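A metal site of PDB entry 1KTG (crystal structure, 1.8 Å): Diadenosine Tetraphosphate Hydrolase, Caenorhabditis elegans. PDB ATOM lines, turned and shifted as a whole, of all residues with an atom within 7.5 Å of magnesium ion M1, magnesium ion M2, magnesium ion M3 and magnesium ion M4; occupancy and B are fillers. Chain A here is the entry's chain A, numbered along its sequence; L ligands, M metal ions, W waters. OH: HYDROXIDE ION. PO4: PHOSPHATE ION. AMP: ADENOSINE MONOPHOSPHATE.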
ATOM      1  N   ALA A   6      27.370 -34.754  24.346  1.00  0.00           N
ATOM      2  CA  ALA A   6      26.096 -34.719  25.031  1.00  0.00           C
ATOM      3  C   ALA A   6      25.307 -33.502  24.616  1.00  0.00           C
ATOM      4  O   ALA A   6      25.849 -32.525  24.128  1.00  0.00           O
ATOM      5  CB  ALA A   6      26.306 -34.702  26.504  1.00  0.00           C
ATOM      6  N   LEU A  23      18.419 -27.879  15.320  1.00  0.00           N
ATOM      7  CA  LEU A  23      19.381 -26.923  14.757  1.00  0.00           C
ATOM      8  C   LEU A  23      20.077 -27.512  13.521  1.00  0.00           C
ATOM      9  O   LEU A  23      20.484 -28.676  13.500  1.00  0.00           O
ATOM     10  CB  LEU A  23      20.449 -26.566  15.789  1.00  0.00           C
ATOM     11  CG  LEU A  23      19.993 -26.197  17.197  1.00  0.00           C
ATOM     12  CD1 LEU A  23      21.221 -25.899  18.040  1.00  0.00           C
ATOM     13  CD2 LEU A  23      19.055 -25.001  17.174  1.00  0.00           C
ATOM     14  N   THR A  33      20.204 -31.602  14.452  1.00  0.00           N
ATOM     15  CA  THR A  33      20.186 -32.280  15.742  1.00  0.00           C
ATOM     16  C   THR A  33      19.755 -31.262  16.784  1.00  0.00           C
ATOM     17  O   THR A  33      19.741 -30.060  16.515  1.00  0.00           O
ATOM     18  CB  THR A  33      21.577 -32.798  16.157  1.00  0.00           C
ATOM     19  OG1 THR A  33      22.364 -31.708  16.645  1.00  0.00           O
ATOM     20  CG2 THR A  33      22.364 -33.386  14.983  1.00  0.00           C
ATOM     21  N   PRO A  34      19.386 -31.731  17.976  1.00  0.00           N
ATOM     22  CA  PRO A  34      19.134 -30.807  19.078  1.00  0.00           C
ATOM     23  C   PRO A  34      20.483 -30.224  19.475  1.00  0.00           C
ATOM     24  O   PRO A  34      21.501 -30.711  18.967  1.00  0.00           O
ATOM     25  CB  PRO A  34      18.573 -31.723  20.192  1.00  0.00           C
ATOM     26  CG  PRO A  34      18.173 -32.970  19.489  1.00  0.00           C
ATOM     27  CD  PRO A  34      19.168 -33.134  18.370  1.00  0.00           C
ATOM     28  N   PRO A  35      20.514 -29.212  20.333  1.00  0.00           N
ATOM     29  CA  PRO A  35      21.791 -28.621  20.753  1.00  0.00           C
ATOM     30  C   PRO A  35      22.633 -29.697  21.422  1.00  0.00           C
ATOM     31  O   PRO A  35      22.136 -30.382  22.283  1.00  0.00           O
ATOM     32  CB  PRO A  35      21.372 -27.549  21.767  1.00  0.00           C
ATOM     33  CG  PRO A  35      19.894 -27.311  21.494  1.00  0.00           C
ATOM     34  CD  PRO A  35      19.366 -28.574  20.971  1.00  0.00           C
ATOM     35  N   LYS A  36      23.894 -29.847  21.011  1.00  0.00           N
ATOM     36  CA  LYS A  36      24.748 -30.889  21.578  1.00  0.00           C
ATOM     37  C   LYS A  36      26.182 -30.696  21.132  1.00  0.00           C
ATOM     38  O   LYS A  36      26.440 -30.076  20.109  1.00  0.00           O
ATOM     39  CB  LYS A  36      24.267 -32.272  21.152  1.00  0.00           C
ATOM     40  CG  LYS A  36      24.359 -32.522  19.662  1.00  0.00           C
ATOM     41  CD  LYS A  36      25.652 -33.202  19.252  1.00  0.00           C
ATOM     42  CE  LYS A  36      25.599 -33.698  17.795  1.00  0.00           C
ATOM     43  NZ  LYS A  36      25.436 -32.612  16.773  1.00  0.00           N
ATOM     44  N   GLY A  37      27.124 -31.258  21.883  1.00  0.00           N
ATOM     45  CA  GLY A  37      28.518 -31.098  21.506  1.00  0.00           C
ATOM     46  C   GLY A  37      29.445 -31.981  22.318  1.00  0.00           C
ATOM     47  O   GLY A  37      29.039 -32.724  23.205  1.00  0.00           O
ATOM     48  N   HIS A  38      30.731 -31.900  21.985  1.00  0.00           N
ATOM     49  CA  HIS A  38      31.696 -32.748  22.646  1.00  0.00           C
ATOM     50  C   HIS A  38      31.860 -32.364  24.101  1.00  0.00           C
ATOM     51  O   HIS A  38      31.749 -31.185  24.473  1.00  0.00           O
ATOM     52  CB  HIS A  38      33.054 -32.656  21.958  1.00  0.00           C
ATOM     53  CG  HIS A  38      33.069 -33.232  20.581  1.00  0.00           C
ATOM     54  ND1 HIS A  38      32.955 -34.592  20.337  1.00  0.00           N
ATOM     55  CD2 HIS A  38      33.214 -32.649  19.367  1.00  0.00           C
ATOM     56  CE1 HIS A  38      33.015 -34.810  19.040  1.00  0.00           C
ATOM     57  NE2 HIS A  38      33.180 -33.659  18.427  1.00  0.00           N
ATOM     58  N   VAL A  39      32.144 -33.370  24.922  1.00  0.00           N
ATOM     59  CA  VAL A  39      32.480 -33.153  26.303  1.00  0.00           C
ATOM     60  C   VAL A  39      33.885 -32.520  26.285  1.00  0.00           C
ATOM     61  O   VAL A  39      34.816 -33.074  25.701  1.00  0.00           O
ATOM     62  CB  VAL A  39      32.459 -34.477  27.105  1.00  0.00           C
ATOM     63  CG1 VAL A  39      32.903 -34.260  28.535  1.00  0.00           C
ATOM     64  CG2 VAL A  39      31.063 -35.049  27.089  1.00  0.00           C
ATOM     65  N   ASP A  40      34.007 -31.336  26.888  1.00  0.00           N
ATOM     66  CA  ASP A  40      35.271 -30.609  26.888  1.00  0.00           C
ATOM     67  C   ASP A  40      36.069 -30.976  28.149  1.00  0.00           C
ATOM     68  O   ASP A  40      35.538 -31.567  29.078  1.00  0.00           O
ATOM     69  CB  ASP A  40      35.007 -29.089  26.805  1.00  0.00           C
ATOM     70  CG  ASP A  40      34.712 -28.602  25.367  1.00  0.00           C
ATOM     71  OD1 ASP A  40      34.890 -29.360  24.394  1.00  0.00           O
ATOM     72  OD2 ASP A  40      34.305 -27.436  25.121  1.00  0.00           O
ATOM     73  N   GLU A  43      34.925 -31.637  32.018  1.00  0.00           N
ATOM     74  CA  GLU A  43      33.467 -31.783  32.080  1.00  0.00           C
ATOM     75  C   GLU A  43      33.001 -33.230  32.092  1.00  0.00           C
ATOM     76  O   GLU A  43      33.727 -34.133  31.709  1.00  0.00           O
ATOM     77  CB  GLU A  43      32.794 -31.119  30.877  1.00  0.00           C
ATOM     78  CG  GLU A  43      33.005 -29.609  30.767  1.00  0.00           C
ATOM     79  CD  GLU A  43      32.245 -29.004  29.598  1.00  0.00           C
ATOM     80  OE1 GLU A  43      32.006 -29.718  28.605  1.00  0.00           O
ATOM     81  OE2 GLU A  43      31.874 -27.817  29.690  1.00  0.00           O
ATOM     82  N   ALA A  48      28.474 -30.735  29.754  1.00  0.00           N
ATOM     83  CA  ALA A  48      28.646 -30.498  28.326  1.00  0.00           C
ATOM     84  C   ALA A  48      27.307 -30.181  27.653  1.00  0.00           C
ATOM     85  O   ALA A  48      27.192 -29.232  26.873  1.00  0.00           O
ATOM     86  CB  ALA A  48      29.306 -31.704  27.688  1.00  0.00           C
ATOM     87  N   ARG A  51      26.243 -26.640  28.634  1.00  0.00           N
ATOM     88  CA  ARG A  51      27.080 -25.603  28.030  1.00  0.00           C
ATOM     89  C   ARG A  51      26.839 -25.504  26.529  1.00  0.00           C
ATOM     90  O   ARG A  51      26.757 -24.416  25.964  1.00  0.00           O
ATOM     91  CB  ARG A  51      28.563 -25.870  28.316  1.00  0.00           C
ATOM     92  CG  ARG A  51      29.505 -24.910  27.586  1.00  0.00           C
ATOM     93  CD  ARG A  51      30.967 -25.280  27.695  1.00  0.00           C
ATOM     94  NE  ARG A  51      31.149 -26.701  27.424  1.00  0.00           N
ATOM     95  CZ  ARG A  51      31.085 -27.250  26.215  1.00  0.00           C
ATOM     96  NH1 ARG A  51      30.874 -26.489  25.153  1.00  0.00           N
ATOM     97  NH2 ARG A  51      31.235 -28.566  26.074  1.00  0.00           N
ATOM     98  N   GLU A  52      26.746 -26.647  25.858  1.00  0.00           N
ATOM     99  CA  GLU A  52      26.512 -26.637  24.414  1.00  0.00           C
ATOM    100  C   GLU A  52      25.138 -26.064  24.088  1.00  0.00           C
ATOM    101  O   GLU A  52      24.955 -25.411  23.065  1.00  0.00           O
ATOM    102  CB  GLU A  52      26.659 -28.054  23.850  1.00  0.00           C
ATOM    103  CG  GLU A  52      28.098 -28.558  23.847  1.00  0.00           C
ATOM    104  CD  GLU A  52      28.946 -28.001  22.709  1.00  0.00           C
ATOM    105  OE1 GLU A  52      28.382 -27.475  21.726  1.00  0.00           O
ATOM    106  OE2 GLU A  52      30.192 -28.114  22.791  1.00  0.00           O
ATOM    107  N   THR A  53      24.182 -26.299  24.972  1.00  0.00           N
ATOM    108  CA  THR A  53      22.862 -25.731  24.758  1.00  0.00           C
ATOM    109  C   THR A  53      22.934 -24.215  24.828  1.00  0.00           C
ATOM    110  O   THR A  53      22.339 -23.512  23.993  1.00  0.00           O
ATOM    111  CB  THR A  53      21.886 -26.275  25.773  1.00  0.00           C
ATOM    112  OG1 THR A  53      21.640 -27.654  25.455  1.00  0.00           O
ATOM    113  CG2 THR A  53      20.536 -25.597  25.659  1.00  0.00           C
ATOM    114  N   GLU A  55      25.599 -22.382  24.335  1.00  0.00           N
ATOM    115  CA  GLU A  55      26.410 -21.913  23.217  1.00  0.00           C
ATOM    116  C   GLU A  55      25.690 -21.937  21.874  1.00  0.00           C
ATOM    117  O   GLU A  55      25.810 -20.993  21.092  1.00  0.00           O
ATOM    118  CB  GLU A  55      27.684 -22.765  23.069  1.00  0.00           C
ATOM    119  CG  GLU A  55      28.762 -22.488  24.099  1.00  0.00           C
ATOM    120  CD  GLU A  55      29.958 -23.423  23.969  1.00  0.00           C
ATOM    121  OE1 GLU A  55      30.009 -24.209  23.008  1.00  0.00           O
ATOM    122  OE2 GLU A  55      30.833 -23.390  24.851  1.00  0.00           O
ATOM    123  N   GLU A  56      24.960 -23.011  21.606  1.00  0.00           N
ATOM    124  CA  GLU A  56      24.374 -23.212  20.286  1.00  0.00           C
ATOM    125  C   GLU A  56      22.993 -22.608  20.087  1.00  0.00           C
ATOM    126  O   GLU A  56      22.605 -22.275  18.961  1.00  0.00           O
ATOM    127  CB  GLU A  56      24.361 -24.704  19.938  1.00  0.00           C
ATOM    128  CG  GLU A  56      25.753 -25.318  19.916  1.00  0.00           C
ATOM    129  CD  GLU A  56      25.768 -26.780  19.517  1.00  0.00           C
ATOM    130  OE1 GLU A  56      24.691 -27.414  19.408  1.00  0.00           O
ATOM    131  OE2 GLU A  56      26.887 -27.301  19.292  1.00  0.00           O
ATOM    132  N   LYS A  83      31.301 -42.534  18.316  1.00  0.00           N
ATOM    133  CA  LYS A  83      30.986 -41.342  19.070  1.00  0.00           C
ATOM    134  C   LYS A  83      29.718 -41.673  19.835  1.00  0.00           C
ATOM    135  O   LYS A  83      28.843 -42.357  19.318  1.00  0.00           O
ATOM    136  CB  LYS A  83      30.738 -40.185  18.120  1.00  0.00           C
ATOM    137  CG  LYS A  83      30.269 -38.899  18.766  1.00  0.00           C
ATOM    138  CD  LYS A  83      30.257 -37.796  17.701  1.00  0.00           C
ATOM    139  CE  LYS A  83      29.755 -36.475  18.191  1.00  0.00           C
ATOM    140  NZ  LYS A  83      30.004 -35.425  17.165  1.00  0.00           N
ATOM    141  N   SER A 101      24.843 -19.722  16.905  1.00  0.00           N
ATOM    142  CA  SER A 101      26.251 -19.405  16.860  1.00  0.00           C
ATOM    143  C   SER A 101      26.739 -19.791  15.461  1.00  0.00           C
ATOM    144  O   SER A 101      25.946 -20.227  14.631  1.00  0.00           O
ATOM    145  CB  SER A 101      26.994 -20.231  17.910  1.00  0.00           C
ATOM    146  OG  SER A 101      27.043 -21.588  17.531  1.00  0.00           O
ATOM    147  N   HIS A 102      28.031 -19.656  15.187  1.00  0.00           N
ATOM    148  CA  HIS A 102      28.567 -19.991  13.868  1.00  0.00           C
ATOM    149  C   HIS A 102      28.407 -21.467  13.514  1.00  0.00           C
ATOM    150  O   HIS A 102      28.513 -21.810  12.342  1.00  0.00           O
ATOM    151  CB  HIS A 102      30.039 -19.608  13.745  1.00  0.00           C
ATOM    152  CG  HIS A 102      30.949 -20.399  14.628  1.00  0.00           C
ATOM    153  ND1 HIS A 102      31.383 -21.666  14.298  1.00  0.00           N
ATOM    154  CD2 HIS A 102      31.541 -20.087  15.807  1.00  0.00           C
ATOM    155  CE1 HIS A 102      32.176 -22.119  15.257  1.00  0.00           C
ATOM    156  NE2 HIS A 102      32.292 -21.175  16.182  1.00  0.00           N
ATOM    157  N   GLU A 103      28.137 -22.317  14.506  1.00  0.00           N
ATOM    158  CA  GLU A 103      27.988 -23.759  14.252  1.00  0.00           C
ATOM    159  C   GLU A 103      26.678 -24.166  13.569  1.00  0.00           C
ATOM    160  O   GLU A 103      26.571 -25.287  13.066  1.00  0.00           O
ATOM    161  CB  GLU A 103      28.205 -24.547  15.548  1.00  0.00           C
ATOM    162  CG  GLU A 103      29.664 -24.499  16.008  1.00  0.00           C
ATOM    163  CD  GLU A 103      29.982 -25.406  17.181  1.00  0.00           C
ATOM    164  OE1 GLU A 103      29.055 -25.901  17.852  1.00  0.00           O
ATOM    165  OE2 GLU A 103      31.188 -25.605  17.405  1.00  0.00           O
ATOM    166  N   HIS A 104      25.698 -23.265  13.538  1.00  0.00           N
ATOM    167  CA  HIS A 104      24.388 -23.544  12.939  1.00  0.00           C
ATOM    168  C   HIS A 104      23.877 -22.403  12.071  1.00  0.00           C
ATOM    169  O   HIS A 104      24.259 -21.248  12.252  1.00  0.00           O
ATOM    170  CB  HIS A 104      23.388 -23.946  14.023  1.00  0.00           C
ATOM    171  CG  HIS A 104      23.824 -25.159  14.769  1.00  0.00           C
ATOM    172  ND1 HIS A 104      24.687 -25.083  15.847  1.00  0.00           N
ATOM    173  CD2 HIS A 104      23.625 -26.480  14.541  1.00  0.00           C
ATOM    174  CE1 HIS A 104      24.972 -26.304  16.258  1.00  0.00           C
ATOM    175  NE2 HIS A 104      24.342 -27.167  15.487  1.00  0.00           N
HETATM  176  O    OH L   1      30.972 -26.620  20.190  1.00  0.00           O
HETATM  177  P   PO4 L   2      30.464 -29.453  18.967  1.00  0.00           P
HETATM  178  O1  PO4 L   2      29.121 -28.769  19.142  1.00  0.00           O
HETATM  179  O2  PO4 L   2      31.354 -28.590  18.085  1.00  0.00           O
HETATM  180  O3  PO4 L   2      31.115 -29.641  20.317  1.00  0.00           O
HETATM  181  O4  PO4 L   2      30.203 -30.785  18.275  1.00  0.00           O
HETATM  182  P   AMP L   3      27.559 -34.508  14.627  1.00  0.00           P
HETATM  183  O1P AMP L   3      26.184 -33.870  14.616  1.00  0.00           O
HETATM  184  O2P AMP L   3      27.616 -35.618  15.654  1.00  0.00           O
HETATM  185  O3P AMP L   3      28.594 -33.429  14.723  1.00  0.00           O
HETATM  186  O5' AMP L   3      27.734 -35.184  13.179  1.00  0.00           O
HETATM  187  C5' AMP L   3      28.948 -35.805  12.790  1.00  0.00           C
HETATM  188  C4' AMP L   3      28.681 -36.640  11.552  1.00  0.00           C
HETATM  189  O4' AMP L   3      27.847 -37.722  11.932  1.00  0.00           O
HETATM  190  C3' AMP L   3      27.949 -35.846  10.473  1.00  0.00           C
HETATM  191  O3' AMP L   3      28.504 -36.159   9.204  1.00  0.00           O
HETATM  192  C2' AMP L   3      26.498 -36.296  10.588  1.00  0.00           C
HETATM  193  O2' AMP L   3      25.867 -36.431   9.326  1.00  0.00           O
HETATM  194  C1' AMP L   3      26.577 -37.646  11.279  1.00  0.00           C
HETATM  195  N9  AMP L   3      25.497 -37.889  12.267  1.00  0.00           N
HETATM  196  C8  AMP L   3      24.932 -37.006  13.114  1.00  0.00           C
HETATM  197  N7  AMP L   3      23.985 -37.630  13.864  1.00  0.00           N
HETATM  198  C5  AMP L   3      23.949 -38.912  13.510  1.00  0.00           C
HETATM  199  C6  AMP L   3      23.172 -40.098  13.915  1.00  0.00           C
HETATM  200  N6  AMP L   3      22.222 -40.007  14.883  1.00  0.00           N
HETATM  201  N1  AMP L   3      23.421 -41.266  13.298  1.00  0.00           N
HETATM  202  C2  AMP L   3      24.369 -41.371  12.331  1.00  0.00           C
HETATM  203  N3  AMP L   3      25.108 -40.310  11.920  1.00  0.00           N
HETATM  204  C4  AMP L   3      24.944 -39.093  12.457  1.00  0.00           C
HETATM  205 MG    MG M   1      28.859 -26.856  19.802  1.00  0.00          MG
HETATM  206 MG    MG M   2      27.207 -29.161  18.456  1.00  0.00          MG
HETATM  207 MG    MG M   3      31.705 -28.172  21.437  1.00  0.00          MG
HETATM  208 MG    MG M   4      32.226 -26.875  18.661  1.00  0.00          MG
HETATM  209  O   HOH W   1      33.479 -28.009  20.163  1.00  0.00           O
HETATM  210  O   HOH W   2      28.785 -24.799  20.547  1.00  0.00           O
HETATM  211  O   HOH W   3      32.631 -26.466  22.677  1.00  0.00           O
HETATM  212  O   HOH W   4      27.727 -28.109  16.671  1.00  0.00           O
HETATM  213  O   HOH W   5      27.767 -30.951  17.486  1.00  0.00           O
HETATM  214  O   HOH W   6      25.248 -29.491  17.689  1.00  0.00           O
HETATM  215  O   HOH W   7      33.750 -27.123  17.155  1.00  0.00           O
HETATM  216  O   HOH W   8      32.839 -29.333  22.661  1.00  0.00           O
HETATM  217  O   HOH W   9      33.292 -24.996  19.327  1.00  0.00           O
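An oxygen (O1P) of AMP L3 is in salt-bridge range of the side-chain amino group (NZ) of Lys 36, at 2.6 Å. The side-chain amino group of Lys 83 is in salt-bridge range of an oxygen (O2P) of AMP L3 (2.8 Å).
The side-chain carboxylate (OE2) of Glu 52 lies close to the guanidinium group (NH1) of Arg 51 (2.9 Å). The backbone carbonyl oxygen (O) of Gly 37 lies within hydrogen-bond range of the backbone NH (N) of Ala 6, at 2.9 Å. The side-chain amino group of Lys 36 sits at hydrogen-bond distance from the side-chain hydroxyl of Thr 33 (3.2 Å). NH2 of Arg 51 is in hydrogen-bond range of O of His 38, 3.1 Å away. The side-chain hydroxyl of Ser 101 lies close to the backbone NH of Glu 103 (3.3 Å).
Of the 22 residues printed, 3 come within 4 Å of magnesium ion M1.
Residues that only touch magnesium ion M2: Gly 37 (3.8 Å). Within 4 Å of magnesium ion M2: Lys 36, Gly 37, Glu 52, Glu 56 and Glu 103. Along chain A the residues within 4 Å of magnesium ion M2 span positions 36 to 103.
Merely in contact with magnesium ion M3: His 38 (3.9 Å). Two residues have an atom within 4 Å of magnesium ion M3: His 38 and Glu 52.
Of the 22 residues printed, 1 comes within 4 Å of magnesium ion M4.
An oxygen (O1) of PO4 L2 binds magnesium ion M1 (2.0 Å). The side-chain carboxylate (OE1) of Glu 52 is bound to magnesium ion M1. OE2 of Glu 56 binds magnesium ion M1. Magnesium ion M1 is bound by O of OH L1, at 2.2 Å. The side-chain carboxylate (OE1) of Glu 103 binds magnesium ion M1 (2.2 Å). Water W2 is bound to magnesium ion M1.
Magnesium ion M2 is bound by the backbone carbonyl oxygen (O) of Lys 36, the side-chain carboxylate (OE2) of Glu 56, an oxygen (O1) of PO4 L2, water W5, water W6 and water W4. Magnesium ion M2 has six donor atoms within binding distance.
Magnesium ion M3 is bound by an oxygen (O3) of PO4 L2 (1.9 Å), the side-chain carboxylate (OE2) of Glu 52 (2.0 Å), water W8 (2.0 Å), an oxygen (O) of OH L1 (2.1 Å), water W1 (2.2 Å) and water W3 (2.3 Å). Magnesium ion M3 has six donor atoms within binding distance.
Magnesium ion M4 is bound by O of OH L1, O2 of PO4 L2, OE2 of Glu 103, water W7, water W9 and water W1.
Water W6 lies within hydrogen-bond range of OE1 of Glu 56, NZ of Lys 36 and NE2 of His 104. Water W3 lies within hydrogen-bond range of NH1 of Arg 51 (3.0 Å), OD2 of Asp 40 (3.1 Å) and OE1 of Glu 55 (3.5 Å). Water W8 bridges the side-chain carboxylate of Asp 40 (2.7 Å) and the backbone carbonyl oxygen of His 38 (2.8 Å).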
